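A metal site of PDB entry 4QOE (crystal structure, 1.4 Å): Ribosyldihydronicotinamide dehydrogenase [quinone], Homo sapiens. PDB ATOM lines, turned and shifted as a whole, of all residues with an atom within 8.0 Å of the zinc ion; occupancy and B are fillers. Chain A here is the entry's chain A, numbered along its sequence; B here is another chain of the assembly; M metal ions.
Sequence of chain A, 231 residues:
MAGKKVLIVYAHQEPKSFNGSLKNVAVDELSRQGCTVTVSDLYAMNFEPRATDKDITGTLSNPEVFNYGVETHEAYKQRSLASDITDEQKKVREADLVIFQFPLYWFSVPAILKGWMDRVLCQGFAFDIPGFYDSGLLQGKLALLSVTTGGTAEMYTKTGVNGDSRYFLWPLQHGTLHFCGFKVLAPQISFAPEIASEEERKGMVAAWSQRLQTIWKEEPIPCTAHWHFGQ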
ATOM      1  N   TYR A 133       9.017 -23.342   4.460  1.00  0.00           N
ATOM      2  CA  TYR A 133       9.203 -22.688   5.739  1.00  0.00           C
ATOM      3  C   TYR A 133       8.640 -21.272   5.692  1.00  0.00           C
ATOM      4  O   TYR A 133       7.499 -21.117   5.413  1.00  0.00           O
ATOM      5  CB  TYR A 133      10.638 -22.856   6.296  1.00  0.00           C
ATOM      6  CG  TYR A 133      10.961 -24.277   6.748  1.00  0.00           C
ATOM      7  CD1 TYR A 133      10.251 -24.900   7.736  1.00  0.00           C
ATOM      8  CD2 TYR A 133      11.955 -24.992   6.147  1.00  0.00           C
ATOM      9  CE1 TYR A 133      10.542 -26.169   8.108  1.00  0.00           C
ATOM     10  CE2 TYR A 133      12.251 -26.268   6.518  1.00  0.00           C
ATOM     11  CZ  TYR A 133      11.531 -26.851   7.513  1.00  0.00           C
ATOM     12  OH  TYR A 133      11.769 -28.117   7.935  1.00  0.00           O
ATOM     13  N   ASP A 134       9.430 -20.242   5.977  1.00  0.00           N
ATOM     14  CA  ASP A 134       8.863 -18.899   6.059  1.00  0.00           C
ATOM     15  C   ASP A 134       8.303 -18.409   4.713  1.00  0.00           C
ATOM     16  O   ASP A 134       7.487 -17.559   4.682  1.00  0.00           O
ATOM     17  CB  ASP A 134       9.860 -17.892   6.612  1.00  0.00           C
ATOM     18  CG  ASP A 134      10.201 -18.137   8.071  1.00  0.00           C
ATOM     19  OD1 ASP A 134       9.526 -18.871   8.765  1.00  0.00           O
ATOM     20  OD2 ASP A 134      11.195 -17.597   8.528  1.00  0.00           O
ATOM     21  N   TRP A 170       7.482 -31.697  17.124  1.00  0.00           N
ATOM     22  CA  TRP A 170       8.393 -31.260  16.041  1.00  0.00           C
ATOM     23  C   TRP A 170       7.994 -31.659  14.624  1.00  0.00           C
ATOM     24  O   TRP A 170       7.917 -30.784  13.759  1.00  0.00           O
ATOM     25  CB  TRP A 170       9.809 -31.733  16.346  1.00  0.00           C
ATOM     26  CG  TRP A 170      10.833 -31.477  15.332  1.00  0.00           C
ATOM     27  CD1 TRP A 170      11.482 -32.402  14.539  1.00  0.00           C
ATOM     28  CD2 TRP A 170      11.474 -30.225  15.087  1.00  0.00           C
ATOM     29  NE1 TRP A 170      12.445 -31.805  13.811  1.00  0.00           N
ATOM     30  CE2 TRP A 170      12.492 -30.452  14.126  1.00  0.00           C
ATOM     31  CE3 TRP A 170      11.303 -28.912  15.598  1.00  0.00           C
ATOM     32  CZ2 TRP A 170      13.327 -29.435  13.669  1.00  0.00           C
ATOM     33  CZ3 TRP A 170      12.108 -27.914  15.129  1.00  0.00           C
ATOM     34  CH2 TRP A 170      13.125 -28.183  14.196  1.00  0.00           C
ATOM     35  N   LEU A 172       5.120 -32.324  13.415  1.00  0.00           N
ATOM     36  CA  LEU A 172       3.840 -31.703  13.091  1.00  0.00           C
ATOM     37  C   LEU A 172       3.968 -30.186  12.935  1.00  0.00           C
ATOM     38  O   LEU A 172       3.627 -29.619  11.904  1.00  0.00           O
ATOM     39  CB  LEU A 172       2.785 -32.039  14.154  1.00  0.00           C
ATOM     40  CG  LEU A 172       2.518 -33.524  14.349  1.00  0.00           C
ATOM     41  CD1 LEU A 172       1.633 -33.819  15.582  1.00  0.00           C
ATOM     42  CD2 LEU A 172       1.905 -34.137  13.081  1.00  0.00           C
ATOM     43  N   GLN A 173       4.454 -29.528  13.985  1.00  0.00           N
ATOM     44  CA  GLN A 173       4.537 -28.093  13.978  1.00  0.00           C
ATOM     45  C   GLN A 173       5.609 -27.639  13.017  1.00  0.00           C
ATOM     46  O   GLN A 173       5.363 -26.703  12.252  1.00  0.00           O
ATOM     47  CB  GLN A 173       4.846 -27.568  15.431  1.00  0.00           C
ATOM     48  CG  GLN A 173       3.651 -27.791  16.339  1.00  0.00           C
ATOM     49  CD  GLN A 173       3.749 -27.101  17.695  1.00  0.00           C
ATOM     50  OE1 GLN A 173       2.715 -26.854  18.329  1.00  0.00           O
ATOM     51  NE2 GLN A 173       4.982 -26.879  18.177  1.00  0.00           N
ATOM     52  N   HIS A 174       6.809 -28.220  13.065  1.00  0.00           N
ATOM     53  CA  HIS A 174       7.883 -27.750  12.237  1.00  0.00           C
ATOM     54  C   HIS A 174       7.924 -28.412  10.860  1.00  0.00           C
ATOM     55  O   HIS A 174       7.895 -27.738   9.850  1.00  0.00           O
ATOM     56  CB  HIS A 174       9.217 -27.905  12.952  1.00  0.00           C
ATOM     57  CG  HIS A 174      10.343 -27.355  12.162  1.00  0.00           C
ATOM     58  ND1 HIS A 174      10.577 -26.015  12.104  1.00  0.00           N
ATOM     59  CD2 HIS A 174      11.317 -27.941  11.455  1.00  0.00           C
ATOM     60  CE1 HIS A 174      11.601 -25.774  11.325  1.00  0.00           C
ATOM     61  NE2 HIS A 174      12.117 -26.932  10.974  1.00  0.00           N
ATOM     62  N   GLY A 175       7.963 -29.732  10.856  1.00  0.00           N
ATOM     63  CA  GLY A 175       8.169 -30.447   9.596  1.00  0.00           C
ATOM     64  C   GLY A 175       6.984 -30.320   8.656  1.00  0.00           C
ATOM     65  O   GLY A 175       7.177 -30.425   7.467  1.00  0.00           O
ATOM     66  N   THR A 176       5.791 -30.018   9.181  1.00  0.00           N
ATOM     67  CA  THR A 176       4.586 -29.963   8.356  1.00  0.00           C
ATOM     68  C   THR A 176       4.058 -28.533   8.304  1.00  0.00           C
ATOM     69  O   THR A 176       4.059 -27.903   7.236  1.00  0.00           O
ATOM     70  CB  THR A 176       3.502 -30.942   8.865  1.00  0.00           C
ATOM     71  OG1 THR A 176       4.074 -32.254   9.062  1.00  0.00           O
ATOM     72  CG2 THR A 176       2.368 -31.044   7.875  1.00  0.00           C
ATOM     73  N   LEU A 177       3.582 -28.012   9.428  1.00  0.00           N
ATOM     74  CA  LEU A 177       2.896 -26.749   9.406  1.00  0.00           C
ATOM     75  C   LEU A 177       3.829 -25.567   9.040  1.00  0.00           C
ATOM     76  O   LEU A 177       3.498 -24.805   8.139  1.00  0.00           O
ATOM     77  CB  LEU A 177       2.154 -26.471  10.700  1.00  0.00           C
ATOM     78  CG  LEU A 177       1.098 -27.520  11.009  1.00  0.00           C
ATOM     79  CD1 LEU A 177       0.541 -27.417  12.433  1.00  0.00           C
ATOM     80  CD2 LEU A 177      -0.064 -27.538   9.999  1.00  0.00           C
ATOM     81  N   HIS A 178       4.940 -25.400   9.767  1.00  0.00           N
ATOM     82  CA  HIS A 178       5.870 -24.354   9.462  1.00  0.00           C
ATOM     83  C   HIS A 178       6.419 -24.551   8.049  1.00  0.00           C
ATOM     84  O   HIS A 178       6.555 -23.571   7.301  1.00  0.00           O
ATOM     85  CB  HIS A 178       6.967 -24.325  10.502  1.00  0.00           C
ATOM     86  CG  HIS A 178       7.929 -23.212  10.368  1.00  0.00           C
ATOM     87  ND1 HIS A 178       9.014 -23.121  11.217  1.00  0.00           N
ATOM     88  CD2 HIS A 178       8.033 -22.130   9.546  1.00  0.00           C
ATOM     89  CE1 HIS A 178       9.735 -22.052  10.926  1.00  0.00           C
ATOM     90  NE2 HIS A 178       9.157 -21.446   9.911  1.00  0.00           N
ATOM     91  N   PHE A 179       6.687 -25.779   7.657  1.00  0.00           N
ATOM     92  CA  PHE A 179       7.165 -26.026   6.312  1.00  0.00           C
ATOM     93  C   PHE A 179       6.258 -25.421   5.253  1.00  0.00           C
ATOM     94  O   PHE A 179       6.725 -24.881   4.250  1.00  0.00           O
ATOM     95  CB  PHE A 179       7.334 -27.538   6.088  1.00  0.00           C
ATOM     96  CG  PHE A 179       8.047 -27.849   4.786  1.00  0.00           C
ATOM     97  CD1 PHE A 179       7.337 -28.003   3.624  1.00  0.00           C
ATOM     98  CD2 PHE A 179       9.415 -27.972   4.738  1.00  0.00           C
ATOM     99  CE1 PHE A 179       7.990 -28.302   2.439  1.00  0.00           C
ATOM    100  CE2 PHE A 179      10.045 -28.287   3.549  1.00  0.00           C
ATOM    101  CZ  PHE A 179       9.341 -28.462   2.391  1.00  0.00           C
ATOM    102  N   PHE A 182       2.678 -21.888   7.591  1.00  0.00           N
ATOM    103  CA  PHE A 182       1.855 -21.478   8.722  1.00  0.00           C
ATOM    104  C   PHE A 182       2.697 -20.850   9.833  1.00  0.00           C
ATOM    105  O   PHE A 182       3.824 -21.274  10.110  1.00  0.00           O
ATOM    106  CB  PHE A 182       1.130 -22.672   9.364  1.00  0.00           C
ATOM    107  CG  PHE A 182       0.004 -23.248   8.580  1.00  0.00           C
ATOM    108  CD1 PHE A 182      -1.275 -22.674   8.680  1.00  0.00           C
ATOM    109  CD2 PHE A 182       0.117 -24.446   7.881  1.00  0.00           C
ATOM    110  CE1 PHE A 182      -2.358 -23.237   8.065  1.00  0.00           C
ATOM    111  CE2 PHE A 182      -0.971 -25.017   7.222  1.00  0.00           C
ATOM    112  CZ  PHE A 182      -2.216 -24.390   7.368  1.00  0.00           C
ATOM    113  N   VAL A 184       2.454 -20.913  13.731  1.00  0.00           N
ATOM    114  CA  VAL A 184       1.996 -21.916  14.653  1.00  0.00           C
ATOM    115  C   VAL A 184       1.661 -21.283  15.996  1.00  0.00           C
ATOM    116  O   VAL A 184       2.545 -20.779  16.710  1.00  0.00           O
ATOM    117  CB  VAL A 184       3.062 -23.030  14.799  1.00  0.00           C
ATOM    118  CG1 VAL A 184       2.579 -24.086  15.783  1.00  0.00           C
ATOM    119  CG2 VAL A 184       3.351 -23.681  13.445  1.00  0.00           C
ATOM    120  N   ILE A 221       4.203 -19.136  18.233  1.00  0.00           N
ATOM    121  CA  ILE A 221       5.497 -19.551  18.783  1.00  0.00           C
ATOM    122  C   ILE A 221       6.606 -19.365  17.809  1.00  0.00           C
ATOM    123  O   ILE A 221       6.409 -19.246  16.595  1.00  0.00           O
ATOM    124  CB  ILE A 221       5.492 -21.009  19.177  1.00  0.00           C
ATOM    125  CG1 ILE A 221       5.522 -21.933  17.909  1.00  0.00           C
ATOM    126  CG2 ILE A 221       4.411 -21.263  20.154  1.00  0.00           C
ATOM    127  CD1 ILE A 221       5.726 -23.415  18.224  1.00  0.00           C
ATOM    128  N   PRO A 222       7.842 -19.338  18.354  1.00  0.00           N
ATOM    129  CA  PRO A 222       8.965 -19.331  17.469  1.00  0.00           C
ATOM    130  C   PRO A 222       9.240 -20.802  17.154  1.00  0.00           C
ATOM    131  O   PRO A 222       9.634 -21.602  18.034  1.00  0.00           O
ATOM    132  CB  PRO A 222      10.095 -18.716  18.339  1.00  0.00           C
ATOM    133  CG  PRO A 222       9.692 -19.026  19.703  1.00  0.00           C
ATOM    134  CD  PRO A 222       8.201 -19.089  19.749  1.00  0.00           C
ATOM    135  N   CYS A 223       8.794 -21.215  15.992  1.00  0.00           N
ATOM    136  CA  CYS A 223       8.792 -22.662  15.690  1.00  0.00           C
ATOM    137  C   CYS A 223      10.202 -23.094  15.232  1.00  0.00           C
ATOM    138  O   CYS A 223      10.521 -23.315  14.017  1.00  0.00           O
ATOM    139  CB  CYS A 223       7.738 -22.991  14.631  1.00  0.00           C
ATOM    140  SG  CYS A 223       7.609 -24.729  14.198  1.00  0.00           S
ATOM    141  N   THR A 224      11.067 -23.236  16.241  1.00  0.00           N
ATOM    142  CA  THR A 224      12.467 -23.494  16.024  1.00  0.00           C
ATOM    143  C   THR A 224      12.888 -24.714  16.797  1.00  0.00           C
ATOM    144  O   THR A 224      12.170 -25.137  17.736  1.00  0.00           O
ATOM    145  CB  THR A 224      13.276 -22.306  16.549  1.00  0.00           C
ATOM    146  OG1 THR A 224      13.124 -22.190  17.985  1.00  0.00           O
ATOM    147  CG2 THR A 224      12.889 -20.992  15.809  1.00  0.00           C
ATOM    148  N   ALA A 225      14.080 -25.227  16.483  1.00  0.00           N
ATOM    149  CA  ALA A 225      14.594 -26.339  17.293  1.00  0.00           C
ATOM    150  C   ALA A 225      14.785 -25.925  18.766  1.00  0.00           C
ATOM    151  O   ALA A 225      14.503 -26.689  19.672  1.00  0.00           O
ATOM    152  CB  ALA A 225      15.901 -26.811  16.717  1.00  0.00           C
ATOM    153  N   TRP A 227      12.958 -23.848  20.540  1.00  0.00           N
ATOM    154  CA  TRP A 227      11.683 -23.898  21.256  1.00  0.00           C
ATOM    155  C   TRP A 227      11.331 -25.350  21.628  1.00  0.00           C
ATOM    156  O   TRP A 227      10.848 -25.620  22.717  1.00  0.00           O
ATOM    157  CB  TRP A 227      10.582 -23.280  20.396  1.00  0.00           C
ATOM    158  CG  TRP A 227       9.240 -23.163  21.091  1.00  0.00           C
ATOM    159  CD1 TRP A 227       8.795 -22.106  21.820  1.00  0.00           C
ATOM    160  CD2 TRP A 227       8.219 -24.112  21.110  1.00  0.00           C
ATOM    161  NE1 TRP A 227       7.540 -22.324  22.310  1.00  0.00           N
ATOM    162  CE2 TRP A 227       7.150 -23.567  21.886  1.00  0.00           C
ATOM    163  CE3 TRP A 227       8.063 -25.377  20.551  1.00  0.00           C
ATOM    164  CZ2 TRP A 227       5.984 -24.234  22.106  1.00  0.00           C
ATOM    165  CZ3 TRP A 227       6.866 -26.051  20.834  1.00  0.00           C
ATOM    166  CH2 TRP A 227       5.862 -25.504  21.575  1.00  0.00           C
ATOM    167  N   HIS A 228      11.540 -26.277  20.680  1.00  0.00           N
ATOM    168  CA  HIS A 228      11.088 -27.661  20.897  1.00  0.00           C
ATOM    169  C   HIS A 228      12.019 -28.446  21.807  1.00  0.00           C
ATOM    170  O   HIS A 228      11.526 -29.275  22.582  1.00  0.00           O
ATOM    171  CB  HIS A 228      10.966 -28.415  19.527  1.00  0.00           C
ATOM    172  CG  HIS A 228       9.823 -27.966  18.678  1.00  0.00           C
ATOM    173  ND1 HIS A 228       9.892 -26.860  17.859  1.00  0.00           N
ATOM    174  CD2 HIS A 228       8.603 -28.494  18.520  1.00  0.00           C
ATOM    175  CE1 HIS A 228       8.712 -26.713  17.254  1.00  0.00           C
ATOM    176  NE2 HIS A 228       7.932 -27.723  17.606  1.00  0.00           N
ATOM    177  N   VAL B 161      18.064 -26.556   8.107  1.00  0.00           N
ATOM    178  CA  VAL B 161      16.595 -26.141   8.129  1.00  0.00           C
ATOM    179  C   VAL B 161      15.601 -27.126   8.754  1.00  0.00           C
ATOM    180  O   VAL B 161      14.557 -26.745   9.362  1.00  0.00           O
ATOM    181  CB  VAL B 161      16.088 -25.664   6.724  1.00  0.00           C
ATOM    182  CG1 VAL B 161      16.837 -24.395   6.320  1.00  0.00           C
ATOM    183  CG2 VAL B 161      16.181 -26.791   5.671  1.00  0.00           C
HETATM  184 ZN    ZN M   1       9.357 -24.491  12.824  1.00  0.00          ZN
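The zinc ion is bound by the backbone carbonyl oxygen of Cys 223 (2.0 Å), a ring nitrogen (ND1) of His 174 (2.1 Å), a ring nitrogen (ND1) of His 178 (2.1 Å) and the side-chain sulfur of Cys 223 (2.2 Å).
SG of Cys 223 lies close to O of Gln 173, 3.6 Å away. OH of Tyr 133 lies within hydrogen-bond range of NE2 of His 174, 3.3 Å away. The backbone carbonyl oxygen (O) of His 174 sits at hydrogen-bond distance from the backbone NH (N) of Phe 179, at 3.2 Å. A ring nitrogen (NE2) of His 174 is in hydrogen-bond range of the backbone carbonyl oxygen (O) of Val 161 of chain B. The backbone NH (N) of His 178 is in hydrogen-bond range of the backbone carbonyl oxygen (O) of Gln 173 (2.8 Å). A ring nitrogen (NE2) of His 178 sits at hydrogen-bond distance from the side-chain carboxylate of Asp 134 (2.8 Å).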
